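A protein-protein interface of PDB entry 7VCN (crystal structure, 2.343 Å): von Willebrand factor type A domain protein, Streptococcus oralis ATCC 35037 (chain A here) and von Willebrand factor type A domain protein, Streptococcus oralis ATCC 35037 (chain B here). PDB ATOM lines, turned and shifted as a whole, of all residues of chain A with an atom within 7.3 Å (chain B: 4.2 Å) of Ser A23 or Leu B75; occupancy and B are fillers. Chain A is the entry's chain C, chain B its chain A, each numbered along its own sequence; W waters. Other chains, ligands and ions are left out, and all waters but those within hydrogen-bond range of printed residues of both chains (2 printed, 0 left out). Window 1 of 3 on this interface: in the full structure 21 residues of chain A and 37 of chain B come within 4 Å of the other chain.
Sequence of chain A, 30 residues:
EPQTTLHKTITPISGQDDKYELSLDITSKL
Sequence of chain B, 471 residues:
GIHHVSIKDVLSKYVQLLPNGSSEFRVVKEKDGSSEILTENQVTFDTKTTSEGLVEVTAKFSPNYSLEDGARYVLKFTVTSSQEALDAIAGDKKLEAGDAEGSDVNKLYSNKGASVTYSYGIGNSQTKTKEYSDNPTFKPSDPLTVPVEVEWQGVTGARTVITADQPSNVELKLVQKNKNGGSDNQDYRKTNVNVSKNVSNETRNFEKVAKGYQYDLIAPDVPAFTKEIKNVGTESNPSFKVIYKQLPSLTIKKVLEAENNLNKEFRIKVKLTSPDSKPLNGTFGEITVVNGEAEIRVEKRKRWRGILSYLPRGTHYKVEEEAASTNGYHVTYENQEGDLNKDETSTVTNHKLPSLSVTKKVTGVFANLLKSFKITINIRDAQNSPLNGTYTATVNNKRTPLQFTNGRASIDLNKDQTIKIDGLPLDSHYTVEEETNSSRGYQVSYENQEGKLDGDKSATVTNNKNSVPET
The side-chain carboxylate of Glu A21 is in salt-bridge range of the guanidinium group of Arg B26, at 3.1 Å. N of Leu A22 sits at hydrogen-bond distance from O of Phe B77, 2.8 Å away. N of Leu B75 lies within hydrogen-bond range of O of Leu A24. The side-chain carboxylate of Asp A25 lies within salt-bridge range of the guanidinium group of Arg B72 (2.8 Å).
Water W2 lies within hydrogen-bond range of OE1 of Glu A21 and NH1 of Arg B26. Water W1 lies within hydrogen-bond range of the side-chain hydroxyl of Ser A23 (2.9 Å), the backbone carbonyl oxygen of His A7 (3.1 Å), the guanidinium group of Arg B72 (3.1 Å) and the side-chain carboxylate of Asp A25 (3.2 Å).
Printed residues of chain A that touch a printed residue of chain B: Glu A21, Leu A22, Ser A23, Leu A24, Asp A25 and Ile A26. Of the 10 printed residues of chain B, 7 touch a printed residue of chain A. Hydrophobic or aromatic side chains of chain B within 4 Å of the printed part of chain A: Ile B7, Val B74, Leu B75 and Phe B77. Among the printed residues, 15 pairs touch across the chains. Among the printed residues, Asp or Glu carboxylates within 4 Å of a Lys or Arg side-chain nitrogen of the other chain: Glu A21 with Arg B26 and Asp A25 with Arg B72.
Among the printed residues, merely in contact across the chains: Ser A23 with Val B74 (3.0 Å), Leu A22 with Lys B76 (3.2 Å), Ser A23 with Leu B75 (3.3 Å), Leu A24 with Val B74 (3.4 Å), Glu A21 with Phe B77 (3.6 Å), Glu A21 with Lys B76 (3.6 Å), Leu A22 with Leu B75 (3.6 Å), Asp A25 with Val B74 (3.7 Å), Ile A26 with Arg B72 (3.7 Å), Leu A24 with Ile B7 (3.9 Å) and Ser A23 with Arg B72 (3.95 Å).
Ser A23 touches three residues of chain B. Of the printed residues of chain B, Leu A24 touches Ile B7 (3.9 Å), Val B74 (3.4 Å) and Leu B75 (2.7 Å). Printed residues of chain B within 4 Å of Asp A25: Arg B72 and Val B74. Of the printed residues of chain A, Arg B26 touches Glu A21. Ala B59 touches none of the printed residues of chain A. Leu B75 touches three residues of chain A. The nearest residue of chain A that does not touch Leu B75 is Asp A25 (4.8 Å). The nearest printed residue of chain A that does not touch Phe B77 is Leu A24 (4.5 Å).
The backbone NH of Asp A25 sits at hydrogen-bond distance from the backbone carbonyl oxygen of His A7. The backbone carbonyl oxygen (O) of Thr A9 lies within hydrogen-bond range of the backbone NH (N) of Ser A23, at 2.9 Å. The backbone carbonyl oxygen of Glu A21 sits at hydrogen-bond distance from the backbone NH of Thr A11 (2.8 Å). The backbone carbonyl oxygen (O) of Ile B7 sits at hydrogen-bond distance from the backbone NH (N) of Ala B59 (2.8 Å). The backbone carbonyl oxygen (O) of Arg B26 lies within hydrogen-bond range of the backbone NH (N) of Lys B76.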
ATOM      1  N   HIS A   7      26.498  -9.079  14.089  1.00  0.00           N
ATOM      2  CA  HIS A   7      26.784  -8.540  12.753  1.00  0.00           C
ATOM      3  C   HIS A   7      25.642  -7.615  12.390  1.00  0.00           C
ATOM      4  O   HIS A   7      24.489  -8.008  12.548  1.00  0.00           O
ATOM      5  CB  HIS A   7      26.891  -9.640  11.682  1.00  0.00           C
ATOM      6  CG  HIS A   7      27.958 -10.634  11.989  1.00  0.00           C
ATOM      7  ND1 HIS A   7      29.319 -10.304  11.951  1.00  0.00           N
ATOM      8  CD2 HIS A   7      27.914 -11.920  12.382  1.00  0.00           C
ATOM      9  CE1 HIS A   7      30.061 -11.335  12.284  1.00  0.00           C
ATOM     10  NE2 HIS A   7      29.218 -12.323  12.590  1.00  0.00           N
ATOM     11  N   LYS A   8      25.988  -6.412  11.924  1.00  0.00           N
ATOM     12  CA  LYS A   8      25.093  -5.389  11.402  1.00  0.00           C
ATOM     13  C   LYS A   8      25.459  -5.064   9.943  1.00  0.00           C
ATOM     14  O   LYS A   8      26.594  -4.693   9.667  1.00  0.00           O
ATOM     15  CB  LYS A   8      25.242  -4.150  12.304  1.00  0.00           C
ATOM     16  CG  LYS A   8      24.392  -2.950  11.878  1.00  0.00           C
ATOM     17  CD  LYS A   8      24.822  -1.664  12.472  1.00  0.00           C
ATOM     18  CE  LYS A   8      23.832  -0.548  12.257  1.00  0.00           C
ATOM     19  NZ  LYS A   8      24.360   0.751  12.723  1.00  0.00           N
ATOM     20  N   THR A   9      24.509  -5.174   8.992  1.00  0.00           N
ATOM     21  CA  THR A   9      24.704  -4.710   7.602  1.00  0.00           C
ATOM     22  C   THR A   9      23.565  -3.770   7.195  1.00  0.00           C
ATOM     23  O   THR A   9      22.491  -3.812   7.823  1.00  0.00           O
ATOM     24  CB  THR A   9      24.640  -5.889   6.603  1.00  0.00           C
ATOM     25  OG1 THR A   9      23.266  -6.225   6.402  1.00  0.00           O
ATOM     26  CG2 THR A   9      25.318  -7.168   7.037  1.00  0.00           C
ATOM     27  N   ILE A  10      23.732  -2.987   6.123  1.00  0.00           N
ATOM     28  CA  ILE A  10      22.602  -2.284   5.486  1.00  0.00           C
ATOM     29  C   ILE A  10      22.543  -2.730   4.023  1.00  0.00           C
ATOM     30  O   ILE A  10      23.562  -2.930   3.387  1.00  0.00           O
ATOM     31  CB  ILE A  10      22.750  -0.751   5.606  1.00  0.00           C
ATOM     32  CG1 ILE A  10      21.489  -0.001   5.188  1.00  0.00           C
ATOM     33  CG2 ILE A  10      23.958  -0.226   4.858  1.00  0.00           C
ATOM     34  CD1 ILE A  10      21.480   1.512   5.513  1.00  0.00           C
ATOM     35  N   THR A  11      21.367  -2.896   3.429  1.00  0.00           N
ATOM     36  CA  THR A  11      21.336  -3.322   2.029  1.00  0.00           C
ATOM     37  C   THR A  11      20.405  -2.410   1.245  1.00  0.00           C
ATOM     38  O   THR A  11      19.270  -2.248   1.656  1.00  0.00           O
ATOM     39  CB  THR A  11      20.776  -4.752   1.950  1.00  0.00           C
ATOM     40  OG1 THR A  11      21.713  -5.522   2.699  1.00  0.00           O
ATOM     41  CG2 THR A  11      20.680  -5.353   0.570  1.00  0.00           C
ATOM     42  N   GLU A  21      17.529  -1.772   3.863  1.00  0.00           N
ATOM     43  CA  GLU A  21      17.128  -2.672   4.932  1.00  0.00           C
ATOM     44  C   GLU A  21      18.272  -2.784   5.908  1.00  0.00           C
ATOM     45  O   GLU A  21      19.386  -3.056   5.453  1.00  0.00           O
ATOM     46  CB  GLU A  21      16.789  -4.052   4.372  1.00  0.00           C
ATOM     47  CG  GLU A  21      16.526  -5.060   5.481  1.00  0.00           C
ATOM     48  CD  GLU A  21      15.572  -6.171   5.037  1.00  0.00           C
ATOM     49  OE1 GLU A  21      14.329  -5.937   4.953  1.00  0.00           O
ATOM     50  OE2 GLU A  21      16.047  -7.308   4.811  1.00  0.00           O
ATOM     51  N   LEU A  22      18.020  -2.491   7.196  1.00  0.00           N
ATOM     52  CA  LEU A  22      19.042  -2.676   8.213  1.00  0.00           C
ATOM     53  C   LEU A  22      18.930  -4.084   8.758  1.00  0.00           C
ATOM     54  O   LEU A  22      17.829  -4.650   8.874  1.00  0.00           O
ATOM     55  CB  LEU A  22      18.905  -1.649   9.323  1.00  0.00           C
ATOM     56  CG  LEU A  22      19.702  -0.371   9.031  1.00  0.00           C
ATOM     57  CD1 LEU A  22      19.155   0.881   9.714  1.00  0.00           C
ATOM     58  CD2 LEU A  22      21.179  -0.547   9.328  1.00  0.00           C
ATOM     59  N   SER A  23      20.066  -4.659   9.134  1.00  0.00           N
ATOM     60  CA  SER A  23      20.003  -6.017   9.660  1.00  0.00           C
ATOM     61  C   SER A  23      20.963  -6.117  10.838  1.00  0.00           C
ATOM     62  O   SER A  23      22.172  -5.967  10.661  1.00  0.00           O
ATOM     63  CB  SER A  23      20.323  -6.996   8.540  1.00  0.00           C
ATOM     64  OG  SER A  23      20.641  -8.268   9.117  1.00  0.00           O
ATOM     65  N   LEU A  24      20.440  -6.260  12.048  1.00  0.00           N
ATOM     66  CA  LEU A  24      21.307  -6.396  13.238  1.00  0.00           C
ATOM     67  C   LEU A  24      21.093  -7.792  13.834  1.00  0.00           C
ATOM     68  O   LEU A  24      19.948  -8.153  14.158  1.00  0.00           O
ATOM     69  CB  LEU A  24      20.995  -5.326  14.300  1.00  0.00           C
ATOM     70  CG  LEU A  24      21.521  -3.918  14.017  1.00  0.00           C
ATOM     71  CD1 LEU A  24      20.731  -3.207  12.936  1.00  0.00           C
ATOM     72  CD2 LEU A  24      21.466  -3.078  15.252  1.00  0.00           C
ATOM     73  N   ASP A  25      22.158  -8.602  13.929  1.00  0.00           N
ATOM     74  CA  ASP A  25      21.929  -9.953  14.406  1.00  0.00           C
ATOM     75  C   ASP A  25      22.709 -10.235  15.692  1.00  0.00           C
ATOM     76  O   ASP A  25      23.592  -9.464  16.053  1.00  0.00           O
ATOM     77  CB  ASP A  25      22.179 -10.969  13.296  1.00  0.00           C
ATOM     78  CG  ASP A  25      23.631 -11.260  13.067  1.00  0.00           C
ATOM     79  OD1 ASP A  25      24.437 -11.171  14.038  1.00  0.00           O
ATOM     80  OD2 ASP A  25      23.938 -11.554  11.935  1.00  0.00           O
ATOM     81  N   ILE A  26      22.361 -11.345  16.341  1.00  0.00           N
ATOM     82  CA  ILE A  26      23.056 -11.906  17.493  1.00  0.00           C
ATOM     83  C   ILE A  26      22.958 -13.430  17.344  1.00  0.00           C
ATOM     84  O   ILE A  26      21.912 -13.942  16.927  1.00  0.00           O
ATOM     85  CB  ILE A  26      22.406 -11.451  18.829  1.00  0.00           C
ATOM     86  CG1 ILE A  26      22.915 -12.241  20.022  1.00  0.00           C
ATOM     87  CG2 ILE A  26      20.907 -11.573  18.790  1.00  0.00           C
ATOM     88  CD1 ILE A  26      23.838 -11.455  20.886  1.00  0.00           C
ATOM     89  N   ILE B   7      18.065  -5.635  21.420  1.00  0.00           N
ATOM     90  CA  ILE B   7      18.961  -5.190  20.369  1.00  0.00           C
ATOM     91  C   ILE B   7      18.584  -3.735  20.100  1.00  0.00           C
ATOM     92  O   ILE B   7      17.383  -3.430  19.991  1.00  0.00           O
ATOM     93  CB  ILE B   7      18.779  -6.021  19.071  1.00  0.00           C
ATOM     94  CG1 ILE B   7      19.138  -7.496  19.184  1.00  0.00           C
ATOM     95  CG2 ILE B   7      19.538  -5.367  17.935  1.00  0.00           C
ATOM     96  CD1 ILE B   7      18.625  -8.335  18.045  1.00  0.00           C
ATOM     97  N   ARG B  26      10.809  -6.623  12.402  1.00  0.00           N
ATOM     98  CA  ARG B  26      10.619  -8.028  12.746  1.00  0.00           C
ATOM     99  C   ARG B  26      11.955  -8.567  13.217  1.00  0.00           C
ATOM    100  O   ARG B  26      12.990  -7.994  12.874  1.00  0.00           O
ATOM    101  CB  ARG B  26      10.116  -8.853  11.552  1.00  0.00           C
ATOM    102  CG  ARG B  26      10.996  -8.788  10.316  1.00  0.00           C
ATOM    103  CD  ARG B  26      10.195  -9.159   9.085  1.00  0.00           C
ATOM    104  NE  ARG B  26      11.187  -9.116   8.001  1.00  0.00           N
ATOM    105  CZ  ARG B  26      11.703  -7.978   7.485  1.00  0.00           C
ATOM    106  NH1 ARG B  26      11.296  -6.781   7.931  1.00  0.00           N
ATOM    107  NH2 ARG B  26      12.636  -8.057   6.537  1.00  0.00           N
ATOM    108  N   VAL B  27      11.925  -9.610  14.047  1.00  0.00           N
ATOM    109  CA  VAL B  27      13.121 -10.383  14.366  1.00  0.00           C
ATOM    110  C   VAL B  27      12.924 -11.802  13.819  1.00  0.00           C
ATOM    111  O   VAL B  27      11.856 -12.397  13.994  1.00  0.00           O
ATOM    112  CB  VAL B  27      13.314 -10.420  15.891  1.00  0.00           C
ATOM    113  CG1 VAL B  27      14.309 -11.489  16.341  1.00  0.00           C
ATOM    114  CG2 VAL B  27      13.594  -9.038  16.458  1.00  0.00           C
ATOM    115  N   PHE B  45       8.744  -3.843  20.058  1.00  0.00           N
ATOM    116  CA  PHE B  45       9.581  -2.829  19.434  1.00  0.00           C
ATOM    117  C   PHE B  45       9.337  -1.470  20.051  1.00  0.00           C
ATOM    118  O   PHE B  45       8.183  -1.095  20.243  1.00  0.00           O
ATOM    119  CB  PHE B  45       9.355  -2.871  17.929  1.00  0.00           C
ATOM    120  CG  PHE B  45       9.652  -4.226  17.325  1.00  0.00           C
ATOM    121  CD1 PHE B  45      10.967  -4.675  17.156  1.00  0.00           C
ATOM    122  CD2 PHE B  45       8.605  -5.084  16.973  1.00  0.00           C
ATOM    123  CE1 PHE B  45      11.210  -5.941  16.633  1.00  0.00           C
ATOM    124  CE2 PHE B  45       8.852  -6.349  16.434  1.00  0.00           C
ATOM    125  CZ  PHE B  45      10.161  -6.775  16.265  1.00  0.00           C
ATOM    126  N   ALA B  59      14.604  -3.649  19.945  1.00  0.00           N
ATOM    127  CA  ALA B  59      13.793  -4.864  19.936  1.00  0.00           C
ATOM    128  C   ALA B  59      14.025  -5.507  21.292  1.00  0.00           C
ATOM    129  O   ALA B  59      15.135  -5.994  21.552  1.00  0.00           O
ATOM    130  CB  ALA B  59      14.233  -5.810  18.821  1.00  0.00           C
ATOM    131  N   ARG B  72      20.642 -17.937  14.775  1.00  0.00           N
ATOM    132  CA  ARG B  72      20.915 -16.549  14.445  1.00  0.00           C
ATOM    133  C   ARG B  72      19.607 -15.774  14.525  1.00  0.00           C
ATOM    134  O   ARG B  72      18.697 -16.018  13.735  1.00  0.00           O
ATOM    135  CB  ARG B  72      21.487 -16.423  13.024  1.00  0.00           C
ATOM    136  CG  ARG B  72      21.824 -15.006  12.575  1.00  0.00           C
ATOM    137  CD  ARG B  72      22.567 -14.967  11.270  1.00  0.00           C
ATOM    138  NE  ARG B  72      22.644 -13.636  10.678  1.00  0.00           N
ATOM    139  CZ  ARG B  72      21.954 -13.151   9.630  1.00  0.00           C
ATOM    140  NH1 ARG B  72      21.057 -13.904   9.028  1.00  0.00           N
ATOM    141  NH2 ARG B  72      22.149 -11.918   9.206  1.00  0.00           N
ATOM    142  N   VAL B  74      17.936 -12.104  13.997  1.00  0.00           N
ATOM    143  CA  VAL B  74      18.290 -10.944  13.191  1.00  0.00           C
ATOM    144  C   VAL B  74      17.115  -9.966  13.180  1.00  0.00           C
ATOM    145  O   VAL B  74      16.005 -10.321  12.767  1.00  0.00           O
ATOM    146  CB  VAL B  74      18.813 -11.352  11.798  1.00  0.00           C
ATOM    147  CG1 VAL B  74      17.881 -12.263  11.049  1.00  0.00           C
ATOM    148  CG2 VAL B  74      19.127 -10.158  10.941  1.00  0.00           C
ATOM    149  N   LEU B  75      17.352  -8.778  13.772  1.00  0.00           N
ATOM    150  CA  LEU B  75      16.403  -7.674  13.715  1.00  0.00           C
ATOM    151  C   LEU B  75      16.491  -7.069  12.306  1.00  0.00           C
ATOM    152  O   LEU B  75      17.584  -6.804  11.807  1.00  0.00           O
ATOM    153  CB  LEU B  75      16.769  -6.633  14.783  1.00  0.00           C
ATOM    154  CG  LEU B  75      16.111  -5.259  14.593  1.00  0.00           C
ATOM    155  CD1 LEU B  75      14.628  -5.361  14.823  1.00  0.00           C
ATOM    156  CD2 LEU B  75      16.706  -4.241  15.531  1.00  0.00           C
ATOM    157  N   LYS B  76      15.358  -6.805  11.671  1.00  0.00           N
ATOM    158  CA  LYS B  76      15.422  -6.233  10.345  1.00  0.00           C
ATOM    159  C   LYS B  76      14.343  -5.169  10.258  1.00  0.00           C
ATOM    160  O   LYS B  76      13.243  -5.356  10.773  1.00  0.00           O
ATOM    161  CB  LYS B  76      15.035  -7.323   9.336  1.00  0.00           C
ATOM    162  CG  LYS B  76      16.048  -8.443   9.090  1.00  0.00           C
ATOM    163  CD  LYS B  76      15.563  -9.139   7.871  1.00  0.00           C
ATOM    164  CE  LYS B  76      16.049 -10.563   7.709  1.00  0.00           C
ATOM    165  NZ  LYS B  76      17.404 -10.445   7.139  1.00  0.00           N
ATOM    166  N   PHE B  77      14.652  -4.044   9.627  1.00  0.00           N
ATOM    167  CA  PHE B  77      13.651  -3.016   9.376  1.00  0.00           C
ATOM    168  C   PHE B  77      14.166  -2.091   8.282  1.00  0.00           C
ATOM    169  O   PHE B  77      15.361  -2.085   8.002  1.00  0.00           O
ATOM    170  CB  PHE B  77      13.385  -2.251  10.659  1.00  0.00           C
ATOM    171  CG  PHE B  77      14.566  -1.545  11.252  1.00  0.00           C
ATOM    172  CD1 PHE B  77      15.453  -2.229  12.078  1.00  0.00           C
ATOM    173  CD2 PHE B  77      14.768  -0.167  11.022  1.00  0.00           C
ATOM    174  CE1 PHE B  77      16.550  -1.557  12.625  1.00  0.00           C
ATOM    175  CE2 PHE B  77      15.878   0.481  11.573  1.00  0.00           C
ATOM    176  CZ  PHE B  77      16.771  -0.221  12.373  1.00  0.00           C
HETATM  177  O   HOH W   1      23.327  -9.128   9.937  1.00  0.00           O
HETATM  178  O   HOH W   2      12.507  -4.541   6.535  1.00  0.00           O
